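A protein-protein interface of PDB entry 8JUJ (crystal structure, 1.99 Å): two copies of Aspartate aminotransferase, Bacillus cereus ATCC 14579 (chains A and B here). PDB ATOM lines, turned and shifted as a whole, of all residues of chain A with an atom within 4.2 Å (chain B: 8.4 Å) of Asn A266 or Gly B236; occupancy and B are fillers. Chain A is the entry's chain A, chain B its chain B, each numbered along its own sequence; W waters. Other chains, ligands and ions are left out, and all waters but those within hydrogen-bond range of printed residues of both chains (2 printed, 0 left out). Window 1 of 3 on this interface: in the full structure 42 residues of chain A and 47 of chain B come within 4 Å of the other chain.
NE2 of Gln B238 sits at hydrogen-bond distance from O of Leu A265 (3.4 Å). The backbone carbonyl oxygen (O) of Phe A55 is in hydrogen-bond range of the backbone NH (N) of Gly B236, 2.9 Å away. The backbone carbonyl oxygen of Asn B233 is in hydrogen-bond range of the backbone NH of Phe A55, 3.4 Å away. The backbone NH (N) of Ala B235 sits at hydrogen-bond distance from the backbone carbonyl oxygen (O) of Phe A55 (3.2 Å). O of Gly B236 lies within hydrogen-bond range of N of Ile A267 (3.0 Å).
OD1 of Asn B266 is in hydrogen-bond range of N of Ala B269, 3.1 Å away. The side-chain amide oxygen (OD1) of Asn A266 sits at hydrogen-bond distance from the backbone NH (N) of Phe A268. The backbone carbonyl oxygen (O) of Leu B237 is in hydrogen-bond range of the side-chain amide nitrogen (ND2) of Asn B266, at 2.9 Å. The side-chain hydroxyl (OH) of Tyr A270 lies within hydrogen-bond range of the backbone NH (N) of Leu A265 (3.1 Å). OD1 of Asp B33 lies within salt-bridge range of NH1 of Arg B10. O of Ser B229 is in hydrogen-bond range of N of Ile B234 (3.0 Å).
Of the 9 printed residues of chain A, 7 touch a printed residue of chain B. Hydrophobic or aromatic side chains of chain A that line the printed part of chain B: Phe A55, Leu A237, Ile A267 and Phe A268. Of the 18 printed residues of chain B, 9 touch a printed residue of chain A. Among the printed residues, 14 pairs touch across the chains. Among the printed residues, no Asp or Glu carboxylate lies within 4 Å of a Lys or Arg side-chain nitrogen of the other chain.
Water W1 lies within hydrogen-bond range of the side-chain amide oxygen (OE1) of Gln B238 (2.9 Å), the side-chain amide nitrogen (ND2) of Asn B266 (3.3 Å) and the side-chain amide nitrogen (ND2) of Asn A266 (3.4 Å). Water W2 lies within hydrogen-bond range of the backbone NH of Gly A56 (3.1 Å) and the guanidinium group of Arg B10 (3.2 Å).
Among the printed residues, pairs that only touch across the chains: Phe A55 with Ile B234, Gly A56 with Asp B33, Gly A56 with Gly B236, Leu A237 with Phe B268, Asn A266 with Gly B236, Asn A266 with Gln B238, Asn A266 with Asn B266, Phe A268 with Leu B237 and Phe A268 with Phe B268.
Asn A266 touches just these residues of chain B: Gly B236, Gln B238 and Asn B266. Of chain A, only Phe A55, Gly A56, Asn A266 and Ile A267 come within 4 Å of Gly B236. Printed residues of chain B within 4 Å of Leu A265: Gln B238. Of the printed residues of chain A, Leu B237 touches Phe A268. Printed residues of chain A within 4 Å of Phe B268: Leu A237 (3.4 Å) and Phe A268 (3.5 Å). Of the printed residues of chain A, Ala B235 touches Phe A55.
Leu A237 touches Phe B268, and with the chains exchanged Phe A268 touches Leu B237. Asn B266 touches its own counterpart, Asn A266. Phe B268 touches its own counterpart, Phe A268. Positions printed for both chains: 237, 265, 266, 267, 268 and 269.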
ATOM      1  N   PHE A  55      -1.405 -21.298 -26.749  1.00  0.00           N
ATOM      2  CA  PHE A  55      -2.359 -22.403 -27.017  1.00  0.00           C
ATOM      3  C   PHE A  55      -1.847 -23.687 -26.342  1.00  0.00           C
ATOM      4  O   PHE A  55      -1.709 -24.685 -27.052  1.00  0.00           O
ATOM      5  CB  PHE A  55      -2.523 -22.519 -28.528  1.00  0.00           C
ATOM      6  CG  PHE A  55      -3.044 -21.248 -29.134  1.00  0.00           C
ATOM      7  CD1 PHE A  55      -4.330 -20.831 -28.866  1.00  0.00           C
ATOM      8  CD2 PHE A  55      -2.232 -20.443 -29.909  1.00  0.00           C
ATOM      9  CE1 PHE A  55      -4.812 -19.642 -29.400  1.00  0.00           C
ATOM     10  CE2 PHE A  55      -2.707 -19.242 -30.427  1.00  0.00           C
ATOM     11  CZ  PHE A  55      -3.994 -18.846 -30.159  1.00  0.00           C
ATOM     12  N   GLY A  56      -1.556 -23.603 -25.036  1.00  0.00           N
ATOM     13  CA  GLY A  56      -1.006 -24.681 -24.207  1.00  0.00           C
ATOM     14  C   GLY A  56      -2.083 -25.581 -23.617  1.00  0.00           C
ATOM     15  O   GLY A  56      -3.279 -25.491 -24.024  1.00  0.00           O
ATOM     16  N   LEU A 237     -14.496 -29.116 -34.941  1.00  0.00           N
ATOM     17  CA  LEU A 237     -13.838 -28.701 -33.685  1.00  0.00           C
ATOM     18  C   LEU A 237     -13.820 -29.860 -32.685  1.00  0.00           C
ATOM     19  O   LEU A 237     -13.144 -29.693 -31.682  1.00  0.00           O
ATOM     20  CB  LEU A 237     -14.568 -27.479 -33.131  1.00  0.00           C
ATOM     21  CG  LEU A 237     -14.641 -26.280 -34.075  1.00  0.00           C
ATOM     22  CD1 LEU A 237     -15.231 -25.086 -33.360  1.00  0.00           C
ATOM     23  CD2 LEU A 237     -13.282 -25.939 -34.631  1.00  0.00           C
ATOM     24  N   LEU A 265     -10.636 -32.188 -24.332  1.00  0.00           N
ATOM     25  CA  LEU A 265     -10.916 -31.591 -25.666  1.00  0.00           C
ATOM     26  C   LEU A 265      -9.839 -30.580 -26.044  1.00  0.00           C
ATOM     27  O   LEU A 265      -9.051 -30.157 -25.171  1.00  0.00           O
ATOM     28  CB  LEU A 265     -12.295 -30.906 -25.664  1.00  0.00           C
ATOM     29  CG  LEU A 265     -13.483 -31.799 -25.334  1.00  0.00           C
ATOM     30  CD1 LEU A 265     -14.814 -31.123 -25.713  1.00  0.00           C
ATOM     31  CD2 LEU A 265     -13.328 -33.123 -26.061  1.00  0.00           C
ATOM     32  N   ASN A 266      -9.769 -30.243 -27.330  1.00  0.00           N
ATOM     33  CA  ASN A 266      -8.851 -29.176 -27.792  1.00  0.00           C
ATOM     34  C   ASN A 266      -9.424 -27.815 -27.328  1.00  0.00           C
ATOM     35  O   ASN A 266     -10.652 -27.716 -27.061  1.00  0.00           O
ATOM     36  CB  ASN A 266      -8.626 -29.260 -29.294  1.00  0.00           C
ATOM     37  CG  ASN A 266      -9.808 -28.730 -30.067  1.00  0.00           C
ATOM     38  OD1 ASN A 266      -9.936 -27.524 -30.223  1.00  0.00           O
ATOM     39  ND2 ASN A 266     -10.645 -29.619 -30.589  1.00  0.00           N
ATOM     40  N   ILE A 267      -8.580 -26.786 -27.293  1.00  0.00           N
ATOM     41  CA  ILE A 267      -8.945 -25.431 -26.790  1.00  0.00           C
ATOM     42  C   ILE A 267     -10.218 -24.963 -27.474  1.00  0.00           C
ATOM     43  O   ILE A 267     -11.090 -24.438 -26.779  1.00  0.00           O
ATOM     44  CB  ILE A 267      -7.807 -24.431 -27.032  1.00  0.00           C
ATOM     45  CG1 ILE A 267      -6.603 -24.764 -26.171  1.00  0.00           C
ATOM     46  CG2 ILE A 267      -8.293 -22.979 -26.843  1.00  0.00           C
ATOM     47  CD1 ILE A 267      -5.308 -24.097 -26.607  1.00  0.00           C
ATOM     48  N   PHE A 268     -10.284 -25.048 -28.799  1.00  0.00           N
ATOM     49  CA  PHE A 268     -11.356 -24.372 -29.561  1.00  0.00           C
ATOM     50  C   PHE A 268     -12.671 -25.137 -29.412  1.00  0.00           C
ATOM     51  O   PHE A 268     -13.725 -24.467 -29.514  1.00  0.00           O
ATOM     52  CB  PHE A 268     -10.922 -24.157 -31.009  1.00  0.00           C
ATOM     53  CG  PHE A 268      -9.834 -23.128 -31.119  1.00  0.00           C
ATOM     54  CD1 PHE A 268     -10.067 -21.814 -30.729  1.00  0.00           C
ATOM     55  CD2 PHE A 268      -8.573 -23.478 -31.575  1.00  0.00           C
ATOM     56  CE1 PHE A 268      -9.059 -20.869 -30.807  1.00  0.00           C
ATOM     57  CE2 PHE A 268      -7.570 -22.527 -31.661  1.00  0.00           C
ATOM     58  CZ  PHE A 268      -7.817 -21.222 -31.284  1.00  0.00           C
ATOM     59  N   ALA A 269     -12.620 -26.444 -29.096  1.00  0.00           N
ATOM     60  CA  ALA A 269     -13.831 -27.247 -28.817  1.00  0.00           C
ATOM     61  C   ALA A 269     -14.519 -26.662 -27.588  1.00  0.00           C
ATOM     62  O   ALA A 269     -15.731 -26.458 -27.644  1.00  0.00           O
ATOM     63  CB  ALA A 269     -13.504 -28.709 -28.609  1.00  0.00           C
ATOM     64  N   TYR A 270     -13.766 -26.422 -26.518  1.00  0.00           N
ATOM     65  CA  TYR A 270     -14.271 -25.806 -25.263  1.00  0.00           C
ATOM     66  C   TYR A 270     -14.831 -24.414 -25.575  1.00  0.00           C
ATOM     67  O   TYR A 270     -15.973 -24.143 -25.153  1.00  0.00           O
ATOM     68  CB  TYR A 270     -13.155 -25.711 -24.228  1.00  0.00           C
ATOM     69  CG  TYR A 270     -12.706 -27.019 -23.620  1.00  0.00           C
ATOM     70  CD1 TYR A 270     -13.620 -27.938 -23.123  1.00  0.00           C
ATOM     71  CD2 TYR A 270     -11.361 -27.324 -23.502  1.00  0.00           C
ATOM     72  CE1 TYR A 270     -13.210 -29.124 -22.525  1.00  0.00           C
ATOM     73  CE2 TYR A 270     -10.932 -28.508 -22.902  1.00  0.00           C
ATOM     74  CZ  TYR A 270     -11.860 -29.412 -22.408  1.00  0.00           C
ATOM     75  OH  TYR A 270     -11.453 -30.592 -21.818  1.00  0.00           O
ATOM     76  N   ARG B  10      -0.748 -15.371 -18.145  1.00  0.00           N
ATOM     77  CA  ARG B  10      -1.573 -16.538 -18.573  1.00  0.00           C
ATOM     78  C   ARG B  10      -2.708 -16.790 -17.577  1.00  0.00           C
ATOM     79  O   ARG B  10      -3.555 -17.659 -17.866  1.00  0.00           O
ATOM     80  CB  ARG B  10      -0.672 -17.760 -18.747  1.00  0.00           C
ATOM     81  CG  ARG B  10       0.352 -17.561 -19.848  1.00  0.00           C
ATOM     82  CD  ARG B  10       1.164 -18.807 -20.076  1.00  0.00           C
ATOM     83  NE  ARG B  10       0.351 -19.917 -20.576  1.00  0.00           N
ATOM     84  CZ  ARG B  10       0.741 -21.200 -20.558  1.00  0.00           C
ATOM     85  NH1 ARG B  10       1.918 -21.534 -20.039  1.00  0.00           N
ATOM     86  NH2 ARG B  10      -0.052 -22.145 -21.034  1.00  0.00           N
ATOM     87  N   ASP B  33       4.383 -26.837 -20.703  1.00  0.00           N
ATOM     88  CA  ASP B  33       4.163 -25.877 -21.818  1.00  0.00           C
ATOM     89  C   ASP B  33       4.948 -24.607 -21.486  1.00  0.00           C
ATOM     90  O   ASP B  33       5.477 -24.549 -20.380  1.00  0.00           O
ATOM     91  CB  ASP B  33       2.674 -25.712 -22.153  1.00  0.00           C
ATOM     92  CG  ASP B  33       1.841 -24.999 -21.094  1.00  0.00           C
ATOM     93  OD1 ASP B  33       2.450 -24.405 -20.188  1.00  0.00           O
ATOM     94  OD2 ASP B  33       0.570 -25.005 -21.213  1.00  0.00           O
ATOM     95  N   ALA B  89      -4.274 -37.374 -32.197  1.00  0.00           N
ATOM     96  CA  ALA B  89      -4.629 -36.152 -31.431  1.00  0.00           C
ATOM     97  C   ALA B  89      -3.814 -36.167 -30.124  1.00  0.00           C
ATOM     98  O   ALA B  89      -4.390 -36.318 -29.039  1.00  0.00           O
ATOM     99  CB  ALA B  89      -6.118 -36.057 -31.206  1.00  0.00           C
ATOM    100  N   PRO B 228       4.233 -30.632 -33.384  1.00  0.00           N
ATOM    101  CA  PRO B 228       4.578 -29.225 -33.154  1.00  0.00           C
ATOM    102  C   PRO B 228       4.164 -28.706 -31.768  1.00  0.00           C
ATOM    103  O   PRO B 228       4.503 -27.587 -31.462  1.00  0.00           O
ATOM    104  CB  PRO B 228       3.795 -28.563 -34.297  1.00  0.00           C
ATOM    105  CG  PRO B 228       2.543 -29.378 -34.365  1.00  0.00           C
ATOM    106  CD  PRO B 228       2.978 -30.805 -34.125  1.00  0.00           C
ATOM    107  N   SER B 229       3.475 -29.533 -30.964  1.00  0.00           N
ATOM    108  CA  SER B 229       2.914 -29.210 -29.620  1.00  0.00           C
ATOM    109  C   SER B 229       3.934 -28.495 -28.740  1.00  0.00           C
ATOM    110  O   SER B 229       3.702 -27.332 -28.375  1.00  0.00           O
ATOM    111  CB  SER B 229       2.424 -30.470 -28.952  1.00  0.00           C
ATOM    112  OG  SER B 229       1.530 -31.135 -29.822  1.00  0.00           O
ATOM    113  N   LYS B 230       5.042 -29.161 -28.421  1.00  0.00           N
ATOM    114  CA  LYS B 230       6.049 -28.623 -27.485  1.00  0.00           C
ATOM    115  C   LYS B 230       6.811 -27.473 -28.158  1.00  0.00           C
ATOM    116  O   LYS B 230       6.935 -26.438 -27.537  1.00  0.00           O
ATOM    117  CB  LYS B 230       7.067 -29.688 -27.072  1.00  0.00           C
ATOM    118  CG  LYS B 230       6.474 -30.869 -26.340  1.00  0.00           C
ATOM    119  CD  LYS B 230       5.562 -30.475 -25.246  1.00  0.00           C
ATOM    120  CE  LYS B 230       5.629 -31.436 -24.090  1.00  0.00           C
ATOM    121  NZ  LYS B 230       4.577 -31.103 -23.109  1.00  0.00           N
ATOM    122  N   ASN B 233       4.464 -24.372 -28.789  1.00  0.00           N
ATOM    123  CA  ASN B 233       3.521 -24.056 -27.687  1.00  0.00           C
ATOM    124  C   ASN B 233       2.071 -24.075 -28.205  1.00  0.00           C
ATOM    125  O   ASN B 233       1.274 -23.167 -27.846  1.00  0.00           O
ATOM    126  CB  ASN B 233       3.919 -22.734 -27.039  1.00  0.00           C
ATOM    127  CG  ASN B 233       3.521 -22.615 -25.587  1.00  0.00           C
ATOM    128  OD1 ASN B 233       3.263 -23.620 -24.913  1.00  0.00           O
ATOM    129  ND2 ASN B 233       3.501 -21.380 -25.092  1.00  0.00           N
ATOM    130  N   ILE B 234       1.682 -25.138 -28.917  1.00  0.00           N
ATOM    131  CA  ILE B 234       0.280 -25.324 -29.409  1.00  0.00           C
ATOM    132  C   ILE B 234      -0.260 -26.699 -28.972  1.00  0.00           C
ATOM    133  O   ILE B 234      -1.100 -27.292 -29.712  1.00  0.00           O
ATOM    134  CB  ILE B 234       0.218 -25.125 -30.931  1.00  0.00           C
ATOM    135  CG1 ILE B 234       1.230 -26.010 -31.670  1.00  0.00           C
ATOM    136  CG2 ILE B 234       0.383 -23.655 -31.298  1.00  0.00           C
ATOM    137  CD1 ILE B 234       0.891 -26.258 -33.120  1.00  0.00           C
ATOM    138  N   ALA B 235       0.159 -27.196 -27.807  1.00  0.00           N
ATOM    139  CA  ALA B 235      -0.242 -28.527 -27.302  1.00  0.00           C
ATOM    140  C   ALA B 235      -1.760 -28.587 -27.151  1.00  0.00           C
ATOM    141  O   ALA B 235      -2.332 -29.672 -27.295  1.00  0.00           O
ATOM    142  CB  ALA B 235       0.425 -28.826 -25.979  1.00  0.00           C
ATOM    143  N   GLY B 236      -2.385 -27.460 -26.815  1.00  0.00           N
ATOM    144  CA  GLY B 236      -3.835 -27.411 -26.599  1.00  0.00           C
ATOM    145  C   GLY B 236      -4.594 -27.633 -27.895  1.00  0.00           C
ATOM    146  O   GLY B 236      -5.830 -27.799 -27.810  1.00  0.00           O
ATOM    147  N   LEU B 237      -3.909 -27.617 -29.043  1.00  0.00           N
ATOM    148  CA  LEU B 237      -4.539 -27.854 -30.375  1.00  0.00           C
ATOM    149  C   LEU B 237      -4.500 -29.332 -30.784  1.00  0.00           C
ATOM    150  O   LEU B 237      -5.161 -29.637 -31.799  1.00  0.00           O
ATOM    151  CB  LEU B 237      -3.887 -26.975 -31.445  1.00  0.00           C
ATOM    152  CG  LEU B 237      -3.935 -25.478 -31.153  1.00  0.00           C
ATOM    153  CD1 LEU B 237      -3.530 -24.679 -32.375  1.00  0.00           C
ATOM    154  CD2 LEU B 237      -5.303 -25.046 -30.648  1.00  0.00           C
ATOM    155  N   GLN B 238      -3.749 -30.188 -30.072  1.00  0.00           N
ATOM    156  CA  GLN B 238      -3.780 -31.670 -30.229  1.00  0.00           C
ATOM    157  C   GLN B 238      -3.423 -32.097 -31.660  1.00  0.00           C
ATOM    158  O   GLN B 238      -4.220 -32.792 -32.334  1.00  0.00           O
ATOM    159  CB  GLN B 238      -5.151 -32.135 -29.780  1.00  0.00           C
ATOM    160  CG  GLN B 238      -5.355 -31.815 -28.312  1.00  0.00           C
ATOM    161  CD  GLN B 238      -6.636 -32.383 -27.778  1.00  0.00           C
ATOM    162  OE1 GLN B 238      -7.522 -32.779 -28.537  1.00  0.00           O
ATOM    163  NE2 GLN B 238      -6.753 -32.368 -26.466  1.00  0.00           N
ATOM    164  N   ALA B 239      -2.263 -31.663 -32.129  1.00  0.00           N
ATOM    165  CA  ALA B 239      -1.718 -32.021 -33.455  1.00  0.00           C
ATOM    166  C   ALA B 239      -0.513 -32.935 -33.252  1.00  0.00           C
ATOM    167  O   ALA B 239       0.441 -32.490 -32.576  1.00  0.00           O
ATOM    168  CB  ALA B 239      -1.337 -30.772 -34.178  1.00  0.00           C
ATOM    169  N   LEU B 265      -7.657 -35.095 -37.198  1.00  0.00           N
ATOM    170  CA  LEU B 265      -7.420 -34.020 -36.216  1.00  0.00           C
ATOM    171  C   LEU B 265      -8.527 -32.986 -36.354  1.00  0.00           C
ATOM    172  O   LEU B 265      -9.236 -33.010 -37.372  1.00  0.00           O
ATOM    173  CB  LEU B 265      -6.055 -33.398 -36.506  1.00  0.00           C
ATOM    174  CG  LEU B 265      -4.880 -34.374 -36.554  1.00  0.00           C
ATOM    175  CD1 LEU B 265      -3.619 -33.634 -36.932  1.00  0.00           C
ATOM    176  CD2 LEU B 265      -4.702 -35.080 -35.222  1.00  0.00           C
ATOM    177  N   ASN B 266      -8.637 -32.079 -35.389  1.00  0.00           N
ATOM    178  CA  ASN B 266      -9.577 -30.937 -35.486  1.00  0.00           C
ATOM    179  C   ASN B 266      -9.005 -29.957 -36.521  1.00  0.00           C
ATOM    180  O   ASN B 266      -7.780 -30.015 -36.837  1.00  0.00           O
ATOM    181  CB  ASN B 266      -9.836 -30.344 -34.094  1.00  0.00           C
ATOM    182  CG  ASN B 266      -8.643 -29.548 -33.617  1.00  0.00           C
ATOM    183  OD1 ASN B 266      -8.444 -28.436 -34.092  1.00  0.00           O
ATOM    184  ND2 ASN B 266      -7.799 -30.134 -32.768  1.00  0.00           N
ATOM    185  N   ILE B 267      -9.841 -29.026 -36.996  1.00  0.00           N
ATOM    186  CA  ILE B 267      -9.507 -28.058 -38.081  1.00  0.00           C
ATOM    187  C   ILE B 267      -8.233 -27.276 -37.747  1.00  0.00           C
ATOM    188  O   ILE B 267      -7.368 -27.101 -38.626  1.00  0.00           O
ATOM    189  CB  ILE B 267     -10.712 -27.125 -38.269  1.00  0.00           C
ATOM    190  CG1 ILE B 267     -11.815 -27.857 -39.016  1.00  0.00           C
ATOM    191  CG2 ILE B 267     -10.314 -25.830 -38.954  1.00  0.00           C
ATOM    192  CD1 ILE B 267     -13.176 -27.188 -38.940  1.00  0.00           C
ATOM    193  N   PHE B 268      -8.129 -26.781 -36.524  1.00  0.00           N
ATOM    194  CA  PHE B 268      -7.061 -25.832 -36.125  1.00  0.00           C
ATOM    195  C   PHE B 268      -5.725 -26.571 -35.933  1.00  0.00           C
ATOM    196  O   PHE B 268      -4.661 -25.956 -36.149  1.00  0.00           O
ATOM    197  CB  PHE B 268      -7.561 -24.994 -34.941  1.00  0.00           C
ATOM    198  CG  PHE B 268      -8.731 -24.105 -35.305  1.00  0.00           C
ATOM    199  CD1 PHE B 268      -8.589 -23.095 -36.244  1.00  0.00           C
ATOM    200  CD2 PHE B 268      -9.967 -24.253 -34.697  1.00  0.00           C
ATOM    201  CE1 PHE B 268      -9.658 -22.264 -36.572  1.00  0.00           C
ATOM    202  CE2 PHE B 268     -11.029 -23.418 -35.020  1.00  0.00           C
ATOM    203  CZ  PHE B 268     -10.880 -22.435 -35.968  1.00  0.00           C
ATOM    204  N   ALA B 269      -5.764 -27.858 -35.589  1.00  0.00           N
ATOM    205  CA  ALA B 269      -4.567 -28.723 -35.557  1.00  0.00           C
ATOM    206  C   ALA B 269      -3.927 -28.679 -36.947  1.00  0.00           C
ATOM    207  O   ALA B 269      -2.720 -28.370 -37.048  1.00  0.00           O
ATOM    208  CB  ALA B 269      -4.920 -30.138 -35.097  1.00  0.00           C
HETATM  209  O   HOH W   1      -9.047 -32.627 -31.052  1.00  0.00           O
HETATM  210  O   HOH W   2      -2.604 -21.637 -22.920  1.00  0.00           O
